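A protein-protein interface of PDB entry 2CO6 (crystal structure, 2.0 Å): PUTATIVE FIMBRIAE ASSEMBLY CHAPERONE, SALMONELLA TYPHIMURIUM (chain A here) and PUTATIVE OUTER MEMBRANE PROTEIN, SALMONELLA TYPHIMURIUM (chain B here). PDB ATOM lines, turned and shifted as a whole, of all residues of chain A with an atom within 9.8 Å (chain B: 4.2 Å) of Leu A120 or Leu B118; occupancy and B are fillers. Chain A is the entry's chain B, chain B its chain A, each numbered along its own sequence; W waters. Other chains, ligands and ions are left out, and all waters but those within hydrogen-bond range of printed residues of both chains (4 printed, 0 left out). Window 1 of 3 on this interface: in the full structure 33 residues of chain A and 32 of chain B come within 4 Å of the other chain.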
ATOM      1  N   ALA A   8      19.683 -15.067  33.009  1.00  0.00           N
ATOM      2  CA  ALA A   8      18.792 -14.427  33.971  1.00  0.00           C
ATOM      3  C   ALA A   8      17.482 -14.020  33.294  1.00  0.00           C
ATOM      4  O   ALA A   8      17.477 -13.659  32.115  1.00  0.00           O
ATOM      5  CB  ALA A   8      19.479 -13.197  34.602  1.00  0.00           C
ATOM      6  N   THR A   9      16.386 -14.095  34.045  1.00  0.00           N
ATOM      7  CA  THR A   9      15.108 -13.490  33.663  1.00  0.00           C
ATOM      8  C   THR A   9      15.216 -11.953  33.567  1.00  0.00           C
ATOM      9  O   THR A   9      15.826 -11.303  34.424  1.00  0.00           O
ATOM     10  CB  THR A   9      13.961 -13.898  34.647  1.00  0.00           C
ATOM     11  OG1 THR A   9      13.731 -15.316  34.558  1.00  0.00           O
ATOM     12  CG2 THR A   9      12.648 -13.196  34.325  1.00  0.00           C
ATOM     13  N   LYS A  10      14.641 -11.387  32.506  1.00  0.00           N
ATOM     14  CA  LYS A  10      14.422  -9.955  32.505  1.00  0.00           C
ATOM     15  C   LYS A  10      13.013  -9.621  32.988  1.00  0.00           C
ATOM     16  O   LYS A  10      12.007 -10.051  32.407  1.00  0.00           O
ATOM     17  CB  LYS A  10      14.690  -9.317  31.149  1.00  0.00           C
ATOM     18  CG  LYS A  10      14.671  -7.795  31.229  1.00  0.00           C
ATOM     19  CD  LYS A  10      15.849  -7.222  32.002  1.00  0.00           C
ATOM     20  CE  LYS A  10      15.677  -5.743  32.198  1.00  0.00           C
ATOM     21  NZ  LYS A  10      16.875  -5.107  32.801  1.00  0.00           N
ATOM     22  N   LEU A  11      12.955  -8.844  34.058  1.00  0.00           N
ATOM     23  CA  LEU A  11      11.692  -8.240  34.459  1.00  0.00           C
ATOM     24  C   LEU A  11      11.749  -6.745  34.188  1.00  0.00           C
ATOM     25  O   LEU A  11      12.729  -6.070  34.499  1.00  0.00           O
ATOM     26  CB  LEU A  11      11.375  -8.536  35.915  1.00  0.00           C
ATOM     27  CG  LEU A  11      10.101  -7.926  36.469  1.00  0.00           C
ATOM     28  CD1 LEU A  11       8.901  -8.703  35.973  1.00  0.00           C
ATOM     29  CD2 LEU A  11      10.146  -7.928  38.000  1.00  0.00           C
ATOM     30  N   PHE A  12      10.733  -6.215  33.534  1.00  0.00           N
ATOM     31  CA  PHE A  12      10.813  -4.779  33.249  1.00  0.00           C
ATOM     32  C   PHE A  12       9.423  -4.167  33.259  1.00  0.00           C
ATOM     33  O   PHE A  12       8.483  -4.754  32.721  1.00  0.00           O
ATOM     34  CB  PHE A  12      11.540  -4.526  31.920  1.00  0.00           C
ATOM     35  CG  PHE A  12      12.007  -3.112  31.748  1.00  0.00           C
ATOM     36  CD1 PHE A  12      12.939  -2.555  32.624  1.00  0.00           C
ATOM     37  CD2 PHE A  12      11.505  -2.332  30.731  1.00  0.00           C
ATOM     38  CE1 PHE A  12      13.353  -1.234  32.469  1.00  0.00           C
ATOM     39  CE2 PHE A  12      11.934  -0.996  30.577  1.00  0.00           C
ATOM     40  CZ  PHE A  12      12.836  -0.466  31.443  1.00  0.00           C
ATOM     41  N   SER A  13       9.302  -2.989  33.873  1.00  0.00           N
ATOM     42  CA  SER A  13       7.999  -2.382  34.069  1.00  0.00           C
ATOM     43  C   SER A  13       8.127  -0.863  34.069  1.00  0.00           C
ATOM     44  O   SER A  13       9.196  -0.337  34.372  1.00  0.00           O
ATOM     45  CB  SER A  13       7.432  -2.865  35.418  1.00  0.00           C
ATOM     46  OG  SER A  13       6.246  -2.133  35.772  1.00  0.00           O
ATOM     47  N   VAL A  14       7.041  -0.171  33.740  1.00  0.00           N
ATOM     48  CA  VAL A  14       6.958   1.293  33.888  1.00  0.00           C
ATOM     49  C   VAL A  14       5.568   1.653  34.395  1.00  0.00           C
ATOM     50  O   VAL A  14       4.595   0.990  34.033  1.00  0.00           O
ATOM     51  CB  VAL A  14       7.338   2.064  32.585  1.00  0.00           C
ATOM     52  CG1 VAL A  14       6.344   1.824  31.458  1.00  0.00           C
ATOM     53  CG2 VAL A  14       7.518   3.596  32.860  1.00  0.00           C
ATOM     54  N   GLN A  38      12.063   0.032  38.775  1.00  0.00           N
ATOM     55  CA  GLN A  38      13.348  -0.620  38.831  1.00  0.00           C
ATOM     56  C   GLN A  38      14.291   0.060  39.823  1.00  0.00           C
ATOM     57  O   GLN A  38      14.204   1.263  40.076  1.00  0.00           O
ATOM     58  CB  GLN A  38      13.978  -0.664  37.433  1.00  0.00           C
ATOM     59  CG  GLN A  38      13.387  -1.788  36.544  1.00  0.00           C
ATOM     60  CD  GLN A  38      12.036  -1.472  35.900  1.00  0.00           C
ATOM     61  OE1 GLN A  38      11.269  -2.382  35.716  1.00  0.00           O
ATOM     62  NE2 GLN A  38      11.754  -0.192  35.546  1.00  0.00           N
ATOM     63  N   TYR A  40      17.291   0.661  39.211  1.00  0.00           N
ATOM     64  CA  TYR A  40      18.350   1.234  38.388  1.00  0.00           C
ATOM     65  C   TYR A  40      17.727   2.259  37.469  1.00  0.00           C
ATOM     66  O   TYR A  40      16.510   2.248  37.282  1.00  0.00           O
ATOM     67  CB  TYR A  40      19.112   0.167  37.592  1.00  0.00           C
ATOM     68  CG  TYR A  40      18.225  -0.804  36.852  1.00  0.00           C
ATOM     69  CD1 TYR A  40      17.694  -0.464  35.619  1.00  0.00           C
ATOM     70  CD2 TYR A  40      17.945  -2.087  37.386  1.00  0.00           C
ATOM     71  CE1 TYR A  40      16.897  -1.304  34.933  1.00  0.00           C
ATOM     72  CE2 TYR A  40      17.166  -2.981  36.694  1.00  0.00           C
ATOM     73  CZ  TYR A  40      16.629  -2.562  35.447  1.00  0.00           C
ATOM     74  OH  TYR A  40      15.845  -3.368  34.664  1.00  0.00           O
ATOM     75  N   ILE A  42      16.432   4.229  34.174  1.00  0.00           N
ATOM     76  CA  ILE A  42      15.909   3.838  32.847  1.00  0.00           C
ATOM     77  C   ILE A  42      15.795   5.050  31.942  1.00  0.00           C
ATOM     78  O   ILE A  42      15.777   6.182  32.416  1.00  0.00           O
ATOM     79  CB  ILE A  42      14.506   3.168  32.972  1.00  0.00           C
ATOM     80  CG1 ILE A  42      13.499   4.165  33.564  1.00  0.00           C
ATOM     81  CG2 ILE A  42      14.629   1.830  33.747  1.00  0.00           C
ATOM     82  CD1 ILE A  42      12.001   3.792  33.506  1.00  0.00           C
ATOM     83  N   LEU A  43      15.769   4.842  30.632  1.00  0.00           N
ATOM     84  CA  LEU A  43      15.573   5.981  29.717  1.00  0.00           C
ATOM     85  C   LEU A  43      14.125   6.045  29.335  1.00  0.00           C
ATOM     86  O   LEU A  43      13.485   5.013  29.089  1.00  0.00           O
ATOM     87  CB  LEU A  43      16.409   5.831  28.425  1.00  0.00           C
ATOM     88  CG  LEU A  43      17.853   5.440  28.667  1.00  0.00           C
ATOM     89  CD1 LEU A  43      18.626   5.307  27.337  1.00  0.00           C
ATOM     90  CD2 LEU A  43      18.494   6.485  29.631  1.00  0.00           C
ATOM     91  N   LYS A  98       7.946   5.296  26.085  1.00  0.00           N
ATOM     92  CA  LYS A  98       8.844   4.162  25.842  1.00  0.00           C
ATOM     93  C   LYS A  98       9.889   4.154  26.941  1.00  0.00           C
ATOM     94  O   LYS A  98      10.497   5.201  27.255  1.00  0.00           O
ATOM     95  CB  LYS A  98       9.536   4.240  24.465  1.00  0.00           C
ATOM     96  CG  LYS A  98      10.699   3.196  24.321  1.00  0.00           C
ATOM     97  CD  LYS A  98      11.577   3.358  23.046  1.00  0.00           C
ATOM     98  CE  LYS A  98      10.780   3.270  21.776  1.00  0.00           C
ATOM     99  NZ  LYS A  98      11.661   2.930  20.588  1.00  0.00           N
ATOM    100  N   ALA A  99      10.095   2.989  27.524  1.00  0.00           N
ATOM    101  CA  ALA A  99      11.073   2.867  28.588  1.00  0.00           C
ATOM    102  C   ALA A  99      12.078   1.815  28.218  1.00  0.00           C
ATOM    103  O   ALA A  99      11.728   0.708  27.725  1.00  0.00           O
ATOM    104  CB  ALA A  99      10.389   2.547  29.947  1.00  0.00           C
ATOM    105  N   VAL A 100      13.335   2.139  28.493  1.00  0.00           N
ATOM    106  CA  VAL A 100      14.440   1.293  28.076  1.00  0.00           C
ATOM    107  C   VAL A 100      15.415   1.182  29.245  1.00  0.00           C
ATOM    108  O   VAL A 100      15.817   2.214  29.801  1.00  0.00           O
ATOM    109  CB  VAL A 100      15.125   1.913  26.782  1.00  0.00           C
ATOM    110  CG1 VAL A 100      16.396   1.176  26.421  1.00  0.00           C
ATOM    111  CG2 VAL A 100      14.163   1.878  25.601  1.00  0.00           C
ATOM    112  N   PRO A 101      15.798  -0.060  29.630  1.00  0.00           N
ATOM    113  CA  PRO A 101      16.773  -0.261  30.690  1.00  0.00           C
ATOM    114  C   PRO A 101      18.214  -0.036  30.169  1.00  0.00           C
ATOM    115  O   PRO A 101      18.411   0.016  28.974  1.00  0.00           O
ATOM    116  CB  PRO A 101      16.593  -1.747  31.014  1.00  0.00           C
ATOM    117  CG  PRO A 101      16.273  -2.377  29.668  1.00  0.00           C
ATOM    118  CD  PRO A 101      15.344  -1.348  29.051  1.00  0.00           C
ATOM    119  N   PRO A 102      19.227   0.002  31.070  1.00  0.00           N
ATOM    120  CA  PRO A 102      20.629  -0.148  30.612  1.00  0.00           C
ATOM    121  C   PRO A 102      20.875  -1.523  29.967  1.00  0.00           C
ATOM    122  O   PRO A 102      20.076  -2.460  30.102  1.00  0.00           O
ATOM    123  CB  PRO A 102      21.467  -0.044  31.898  1.00  0.00           C
ATOM    124  CG  PRO A 102      20.560   0.282  32.979  1.00  0.00           C
ATOM    125  CD  PRO A 102      19.130   0.125  32.532  1.00  0.00           C
ATOM    126  N   GLU A 103      21.983  -1.643  29.255  1.00  0.00           N
ATOM    127  CA  GLU A 103      22.368  -2.935  28.742  1.00  0.00           C
ATOM    128  C   GLU A 103      22.721  -3.728  29.978  1.00  0.00           C
ATOM    129  O   GLU A 103      23.107  -3.136  31.000  1.00  0.00           O
ATOM    130  CB  GLU A 103      23.514  -2.819  27.716  1.00  0.00           C
ATOM    131  CG  GLU A 103      23.009  -2.366  26.294  1.00  0.00           C
ATOM    132  CD  GLU A 103      21.931  -3.313  25.675  1.00  0.00           C
ATOM    133  OE1 GLU A 103      22.301  -4.355  25.080  1.00  0.00           O
ATOM    134  OE2 GLU A 103      20.711  -3.012  25.773  1.00  0.00           O
ATOM    135  N   ASN A 104      22.507  -5.040  29.930  1.00  0.00           N
ATOM    136  CA  ASN A 104      22.808  -5.874  31.088  1.00  0.00           C
ATOM    137  C   ASN A 104      24.322  -5.972  31.323  1.00  0.00           C
ATOM    138  O   ASN A 104      25.114  -5.873  30.389  1.00  0.00           O
ATOM    139  CB  ASN A 104      22.192  -7.283  30.941  1.00  0.00           C
ATOM    140  CG  ASN A 104      20.663  -7.263  30.840  1.00  0.00           C
ATOM    141  OD1 ASN A 104      19.986  -6.474  31.522  1.00  0.00           O
ATOM    142  ND2 ASN A 104      20.110  -8.135  29.985  1.00  0.00           N
ATOM    143  N   ASP A 117      21.363 -13.406  26.872  1.00  0.00           N
ATOM    144  CA  ASP A 117      21.358 -12.142  27.602  1.00  0.00           C
ATOM    145  C   ASP A 117      20.053 -11.464  27.158  1.00  0.00           C
ATOM    146  O   ASP A 117      19.934 -10.895  26.060  1.00  0.00           O
ATOM    147  CB  ASP A 117      22.624 -11.332  27.288  1.00  0.00           C
ATOM    148  CG  ASP A 117      22.556  -9.886  27.782  1.00  0.00           C
ATOM    149  OD1 ASP A 117      21.950  -9.616  28.838  1.00  0.00           O
ATOM    150  OD2 ASP A 117      23.143  -9.003  27.115  1.00  0.00           O
ATOM    151  N   LEU A 118      19.058 -11.601  28.019  1.00  0.00           N
ATOM    152  CA  LEU A 118      17.687 -11.274  27.711  1.00  0.00           C
ATOM    153  C   LEU A 118      17.381  -9.831  28.146  1.00  0.00           C
ATOM    154  O   LEU A 118      17.703  -9.443  29.276  1.00  0.00           O
ATOM    155  CB  LEU A 118      16.826 -12.240  28.501  1.00  0.00           C
ATOM    156  CG  LEU A 118      16.286 -13.532  27.858  1.00  0.00           C
ATOM    157  CD1 LEU A 118      16.738 -13.834  26.422  1.00  0.00           C
ATOM    158  CD2 LEU A 118      16.279 -14.722  28.747  1.00  0.00           C
ATOM    159  N   ASN A 119      16.746  -9.040  27.278  1.00  0.00           N
ATOM    160  CA  ASN A 119      16.440  -7.655  27.644  1.00  0.00           C
ATOM    161  C   ASN A 119      15.149  -7.209  26.950  1.00  0.00           C
ATOM    162  O   ASN A 119      14.652  -7.895  26.047  1.00  0.00           O
ATOM    163  CB  ASN A 119      17.622  -6.718  27.357  1.00  0.00           C
ATOM    164  CG  ASN A 119      17.759  -5.577  28.391  1.00  0.00           C
ATOM    165  OD1 ASN A 119      18.802  -4.892  28.441  1.00  0.00           O
ATOM    166  ND2 ASN A 119      16.742  -5.391  29.226  1.00  0.00           N
ATOM    167  N   LEU A 120      14.567  -6.127  27.441  1.00  0.00           N
ATOM    168  CA  LEU A 120      13.250  -5.674  26.978  1.00  0.00           C
ATOM    169  C   LEU A 120      13.272  -4.182  26.770  1.00  0.00           C
ATOM    170  O   LEU A 120      14.129  -3.487  27.316  1.00  0.00           O
ATOM    171  CB  LEU A 120      12.170  -6.010  28.037  1.00  0.00           C
ATOM    172  CG  LEU A 120      11.864  -7.495  28.296  1.00  0.00           C
ATOM    173  CD1 LEU A 120      11.072  -7.604  29.573  1.00  0.00           C
ATOM    174  CD2 LEU A 120      11.053  -8.084  27.117  1.00  0.00           C
ATOM    175  N   SER A 121      12.326  -3.731  25.964  1.00  0.00           N
ATOM    176  CA  SER A 121      11.996  -2.328  25.753  1.00  0.00           C
ATOM    177  C   SER A 121      10.480  -2.368  25.800  1.00  0.00           C
ATOM    178  O   SER A 121       9.857  -3.285  25.235  1.00  0.00           O
ATOM    179  CB  SER A 121      12.447  -1.847  24.374  1.00  0.00           C
ATOM    180  OG  SER A 121      11.826  -0.616  24.038  1.00  0.00           O
ATOM    181  N   ILE A 122       9.877  -1.431  26.532  1.00  0.00           N
ATOM    182  CA  ILE A 122       8.409  -1.418  26.620  1.00  0.00           C
ATOM    183  C   ILE A 122       7.848  -0.055  26.287  1.00  0.00           C
ATOM    184  O   ILE A 122       8.534   0.956  26.466  1.00  0.00           O
ATOM    185  CB  ILE A 122       7.887  -1.862  28.012  1.00  0.00           C
ATOM    186  CG1 ILE A 122       8.326  -0.873  29.101  1.00  0.00           C
ATOM    187  CG2 ILE A 122       8.337  -3.294  28.306  1.00  0.00           C
ATOM    188  CD1 ILE A 122       8.047  -1.345  30.518  1.00  0.00           C
ATOM    189  N   ASN A 123       6.604  -0.044  25.782  1.00  0.00           N
ATOM    190  CA  ASN A 123       5.936   1.187  25.377  1.00  0.00           C
ATOM    191  C   ASN A 123       4.533   1.169  25.959  1.00  0.00           C
ATOM    192  O   ASN A 123       3.738   0.277  25.653  1.00  0.00           O
ATOM    193  CB  ASN A 123       5.886   1.358  23.834  1.00  0.00           C
ATOM    194  CG  ASN A 123       7.230   1.150  23.154  1.00  0.00           C
ATOM    195  OD1 ASN A 123       7.821   2.105  22.635  1.00  0.00           O
ATOM    196  ND2 ASN A 123       7.697  -0.098  23.103  1.00  0.00           N
ATOM    197  N   VAL B   6       6.504  -6.668  32.021  1.00  0.00           N
ATOM    198  CA  VAL B   6       6.868  -7.694  31.056  1.00  0.00           C
ATOM    199  C   VAL B   6       8.026  -8.523  31.615  1.00  0.00           C
ATOM    200  O   VAL B   6       8.967  -7.967  32.166  1.00  0.00           O
ATOM    201  CB  VAL B   6       7.270  -7.074  29.698  1.00  0.00           C
ATOM    202  CG1 VAL B   6       7.485  -8.165  28.660  1.00  0.00           C
ATOM    203  CG2 VAL B   6       6.208  -6.019  29.204  1.00  0.00           C
ATOM    204  N   LEU B   8      10.765 -11.548  30.426  1.00  0.00           N
ATOM    205  CA  LEU B   8      11.289 -12.458  29.423  1.00  0.00           C
ATOM    206  C   LEU B   8      12.120 -13.502  30.157  1.00  0.00           C
ATOM    207  O   LEU B   8      13.126 -13.156  30.758  1.00  0.00           O
ATOM    208  CB  LEU B   8      12.084 -11.698  28.364  1.00  0.00           C
ATOM    209  CG  LEU B   8      12.676 -12.311  27.108  1.00  0.00           C
ATOM    210  CD1 LEU B   8      11.625 -12.987  26.248  1.00  0.00           C
ATOM    211  CD2 LEU B   8      13.376 -11.152  26.365  1.00  0.00           C
ATOM    212  N   LEU B  28       7.736 -15.311  26.941  1.00  0.00           N
ATOM    213  CA  LEU B  28       7.367 -13.921  27.142  1.00  0.00           C
ATOM    214  C   LEU B  28       6.062 -13.832  27.899  1.00  0.00           C
ATOM    215  O   LEU B  28       5.070 -14.430  27.490  1.00  0.00           O
ATOM    216  CB  LEU B  28       7.233 -13.207  25.788  1.00  0.00           C
ATOM    217  CG  LEU B  28       6.849 -11.716  25.907  1.00  0.00           C
ATOM    218  CD1 LEU B  28       8.015 -10.872  26.413  1.00  0.00           C
ATOM    219  CD2 LEU B  28       6.313 -11.142  24.595  1.00  0.00           C
ATOM    220  N   VAL B  40       4.278  -7.288  19.936  1.00  0.00           N
ATOM    221  CA  VAL B  40       5.693  -7.526  20.204  1.00  0.00           C
ATOM    222  C   VAL B  40       6.480  -7.731  18.922  1.00  0.00           C
ATOM    223  O   VAL B  40       5.998  -8.412  17.969  1.00  0.00           O
ATOM    224  CB  VAL B  40       5.909  -8.723  21.221  1.00  0.00           C
ATOM    225  CG1 VAL B  40       5.394 -10.057  20.661  1.00  0.00           C
ATOM    226  CG2 VAL B  40       7.389  -8.814  21.672  1.00  0.00           C
ATOM    227  N   ARG B  41       7.669  -7.123  18.894  1.00  0.00           N
ATOM    228  CA  ARG B  41       8.646  -7.306  17.806  1.00  0.00           C
ATOM    229  C   ARG B  41      10.003  -7.565  18.452  1.00  0.00           C
ATOM    230  O   ARG B  41      10.300  -6.981  19.498  1.00  0.00           O
ATOM    231  CB  ARG B  41       8.768  -6.036  16.934  1.00  0.00           C
ATOM    232  CG  ARG B  41       7.609  -5.733  15.968  1.00  0.00           C
ATOM    233  CD  ARG B  41       7.838  -4.428  15.154  1.00  0.00           C
ATOM    234  NE  ARG B  41       9.084  -4.496  14.364  1.00  0.00           N
ATOM    235  CZ  ARG B  41       9.179  -4.954  13.114  1.00  0.00           C
ATOM    236  NH1 ARG B  41       8.096  -5.348  12.453  1.00  0.00           N
ATOM    237  NH2 ARG B  41      10.372  -5.014  12.517  1.00  0.00           N
ATOM    238  N   GLY B  42      10.826  -8.422  17.839  1.00  0.00           N
ATOM    239  CA  GLY B  42      12.252  -8.524  18.218  1.00  0.00           C
ATOM    240  C   GLY B  42      12.976  -7.268  17.768  1.00  0.00           C
ATOM    241  O   GLY B  42      12.644  -6.718  16.709  1.00  0.00           O
ATOM    242  N   TRP B  55      14.231 -13.369  13.498  1.00  0.00           N
ATOM    243  CA  TRP B  55      15.429 -12.545  13.274  1.00  0.00           C
ATOM    244  C   TRP B  55      16.673 -13.321  13.678  1.00  0.00           C
ATOM    245  O   TRP B  55      16.578 -14.428  14.246  1.00  0.00           O
ATOM    246  CB  TRP B  55      15.345 -11.194  14.034  1.00  0.00           C
ATOM    247  CG  TRP B  55      15.278 -11.290  15.580  1.00  0.00           C
ATOM    248  CD1 TRP B  55      16.319 -11.098  16.468  1.00  0.00           C
ATOM    249  CD2 TRP B  55      14.119 -11.567  16.387  1.00  0.00           C
ATOM    250  NE1 TRP B  55      15.872 -11.242  17.771  1.00  0.00           N
ATOM    251  CE2 TRP B  55      14.530 -11.519  17.749  1.00  0.00           C
ATOM    252  CE3 TRP B  55      12.776 -11.820  16.097  1.00  0.00           C
ATOM    253  CZ2 TRP B  55      13.643 -11.748  18.804  1.00  0.00           C
ATOM    254  CZ3 TRP B  55      11.905 -12.065  17.126  1.00  0.00           C
ATOM    255  CH2 TRP B  55      12.330 -12.029  18.478  1.00  0.00           C
ATOM    256  N   ILE B 100       9.599 -18.140  22.529  1.00  0.00           N
ATOM    257  CA  ILE B 100      10.683 -17.843  21.595  1.00  0.00           C
ATOM    258  C   ILE B 100      11.455 -19.159  21.399  1.00  0.00           C
ATOM    259  O   ILE B 100      11.754 -19.875  22.364  1.00  0.00           O
ATOM    260  CB  ILE B 100      11.619 -16.750  22.147  1.00  0.00           C
ATOM    261  CG1 ILE B 100      10.836 -15.507  22.614  1.00  0.00           C
ATOM    262  CG2 ILE B 100      12.738 -16.417  21.148  1.00  0.00           C
ATOM    263  CD1 ILE B 100      10.015 -14.795  21.531  1.00  0.00           C
ATOM    264  N   THR B 117      16.620  -9.053  22.487  1.00  0.00           N
ATOM    265  CA  THR B 117      15.776  -7.972  22.997  1.00  0.00           C
ATOM    266  C   THR B 117      14.432  -7.929  22.282  1.00  0.00           C
ATOM    267  O   THR B 117      14.353  -7.970  21.043  1.00  0.00           O
ATOM    268  CB  THR B 117      16.447  -6.595  22.880  1.00  0.00           C
ATOM    269  OG1 THR B 117      17.668  -6.622  23.607  1.00  0.00           O
ATOM    270  CG2 THR B 117      15.553  -5.516  23.484  1.00  0.00           C
ATOM    271  N   LEU B 118      13.371  -7.858  23.069  1.00  0.00           N
ATOM    272  CA  LEU B 118      12.035  -7.741  22.496  1.00  0.00           C
ATOM    273  C   LEU B 118      11.487  -6.386  22.904  1.00  0.00           C
ATOM    274  O   LEU B 118      11.750  -5.919  24.003  1.00  0.00           O
ATOM    275  CB  LEU B 118      11.140  -8.854  23.046  1.00  0.00           C
ATOM    276  CG  LEU B 118      11.524 -10.311  22.791  1.00  0.00           C
ATOM    277  CD1 LEU B 118      10.451 -11.214  23.380  1.00  0.00           C
ATOM    278  CD2 LEU B 118      11.532 -10.538  21.348  1.00  0.00           C
ATOM    279  N   ASP B 119      10.704  -5.788  22.026  1.00  0.00           N
ATOM    280  CA  ASP B 119      10.061  -4.487  22.220  1.00  0.00           C
ATOM    281  C   ASP B 119       8.547  -4.760  22.352  1.00  0.00           C
ATOM    282  O   ASP B 119       7.959  -5.457  21.508  1.00  0.00           O
ATOM    283  CB  ASP B 119      10.325  -3.651  20.967  1.00  0.00           C
ATOM    284  CG  ASP B 119      10.015  -2.192  21.153  1.00  0.00           C
ATOM    285  OD1 ASP B 119       9.888  -1.517  20.096  1.00  0.00           O
ATOM    286  OD2 ASP B 119       9.880  -1.728  22.333  1.00  0.00           O
ATOM    287  N   VAL B 120       7.945  -4.303  23.447  1.00  0.00           N
ATOM    288  CA  VAL B 120       6.554  -4.610  23.733  1.00  0.00           C
ATOM    289  C   VAL B 120       5.764  -3.321  23.810  1.00  0.00           C
ATOM    290  O   VAL B 120       6.204  -2.356  24.453  1.00  0.00           O
ATOM    291  CB  VAL B 120       6.397  -5.432  25.042  1.00  0.00           C
ATOM    292  CG1 VAL B 120       4.973  -5.705  25.378  1.00  0.00           C
ATOM    293  CG2 VAL B 120       7.185  -6.767  24.937  1.00  0.00           C
HETATM  294  O   HOH W   1      12.303   0.441  20.238  1.00  0.00           O
HETATM  295  O   HOH W   2      18.481  -4.377  24.417  1.00  0.00           O
HETATM  296  O   HOH W   3      19.871  -8.338  25.366  1.00  0.00           O
HETATM  297  O   HOH W   4       8.850   0.904  19.971  1.00  0.00           O
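Water W2 bridges OG1 of Thr B117 (2.5 Å) and OE2 of Glu A103 (2.9 Å). Water W1 bridges the side-chain amino group (NZ) of Lys A98 (2.6 Å) and the side-chain carboxylate (OD1) of Asp B119 (3.1 Å). Water W4 lies within hydrogen-bond range of OD1 of Asp B119 (2.6 Å) and OD1 of Asn A123 (3.1 Å). Water W3 lies within hydrogen-bond range of the backbone carbonyl oxygen of Asp A117 and the side-chain hydroxyl of Thr B117.
The backbone NH (N) of Phe A12 is in hydrogen-bond range of the backbone carbonyl oxygen (O) of Val B6 (2.8 Å). N of Leu B8 lies within hydrogen-bond range of O of Lys A10. N of Leu B118 is in hydrogen-bond range of O of Asn A119. The backbone NH of Ser A121 sits at hydrogen-bond distance from the backbone carbonyl oxygen of Leu B118 (3.0 Å). OD2 of Asp B119 is in hydrogen-bond range of OG of Ser A121. ND2 of Asn A123 lies within hydrogen-bond range of OD2 of Asp B119 (2.8 Å). The backbone NH (N) of Val B120 sits at hydrogen-bond distance from the backbone carbonyl oxygen (O) of Ser A121, at 2.8 Å. O of Val B120 is in hydrogen-bond range of N of Asn A123.
Of the 25 printed residues of chain A, 10 touch a printed residue of chain B. Printed residues of chain A that touch a printed residue of chain B: Thr A9, Lys A10, Leu A11, Phe A12, Leu A118, Asn A119, Leu A120, Ser A121, Ile A122 and Asn A123. Of the 12 printed residues of chain B, 6 touch a printed residue of chain A.
Thr A9 touches Leu B8. Lys A10 touches Val B6 (O to O, 3.7 Å). Leu A11 touches Val B6. Leu A118 touches Leu B8. Asn A119 touches Leu B8 (O to CD2, 3.5 Å). Thr B117 touches Asn A119. Val B6 touches Leu A120 (O to CD1, 3.4 Å). Leu B8 touches Leu A120 (CD2 to CD2, 3.9 Å). Leu A120 touches Leu B118 (CA to O, 3.3 Å). Val B120 touches Ile A122.
Of the printed residues of chain B, Thr A9 touches Leu B8. Ile A42 touches none of the printed residues of chain B. Of the printed residues of chain B, Leu A118 touches Leu B8 (3.9 Å). Printed residues of chain B within 4 Å of Asn A119: Leu B8, Thr B117 and Leu B118. Leu A120 touches three residues of chain B. Of the printed residues of chain B, Ile A122 touches Val B6 (3.6 Å) and Val B120 (3.2 Å). Printed residues of chain B within 4 Å of Asn A123: Asp B119 (2.8 Å) and Val B120 (2.7 Å). Of chain A, only Lys A10 (3.7 Å), Leu A11 (3.6 Å), Phe A12 (2.8 Å), Leu A120 (3.4 Å) and Ile A122 (3.6 Å) come within 4 Å of Val B6. Thr B117 touches just one residue of chain A: Asn A119 (3.3 Å). Of chain A, only Asn A119 (3.2 Å), Leu A120 (3.3 Å) and Ser A121 (3.0 Å) come within 4 Å of Leu B118.
The backbone carbonyl oxygen of Arg B41 lies within hydrogen-bond range of the backbone NH of Asp B119, at 2.8 Å. The side-chain amino group (NZ) of Lys A10 lies within hydrogen-bond range of the side-chain hydroxyl (OH) of Tyr A40 (2.7 Å). The backbone carbonyl oxygen (O) of Ile A122 lies within hydrogen-bond range of the backbone NH (N) of Ala A99 (2.8 Å). The backbone carbonyl oxygen (O) of Pro A102 sits close to the side-chain amide oxygen (OD1) of Asn A119 (3.2 Å). ND2 of Asn A104 lies within hydrogen-bond range of O of Leu A118, at 2.8 Å.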
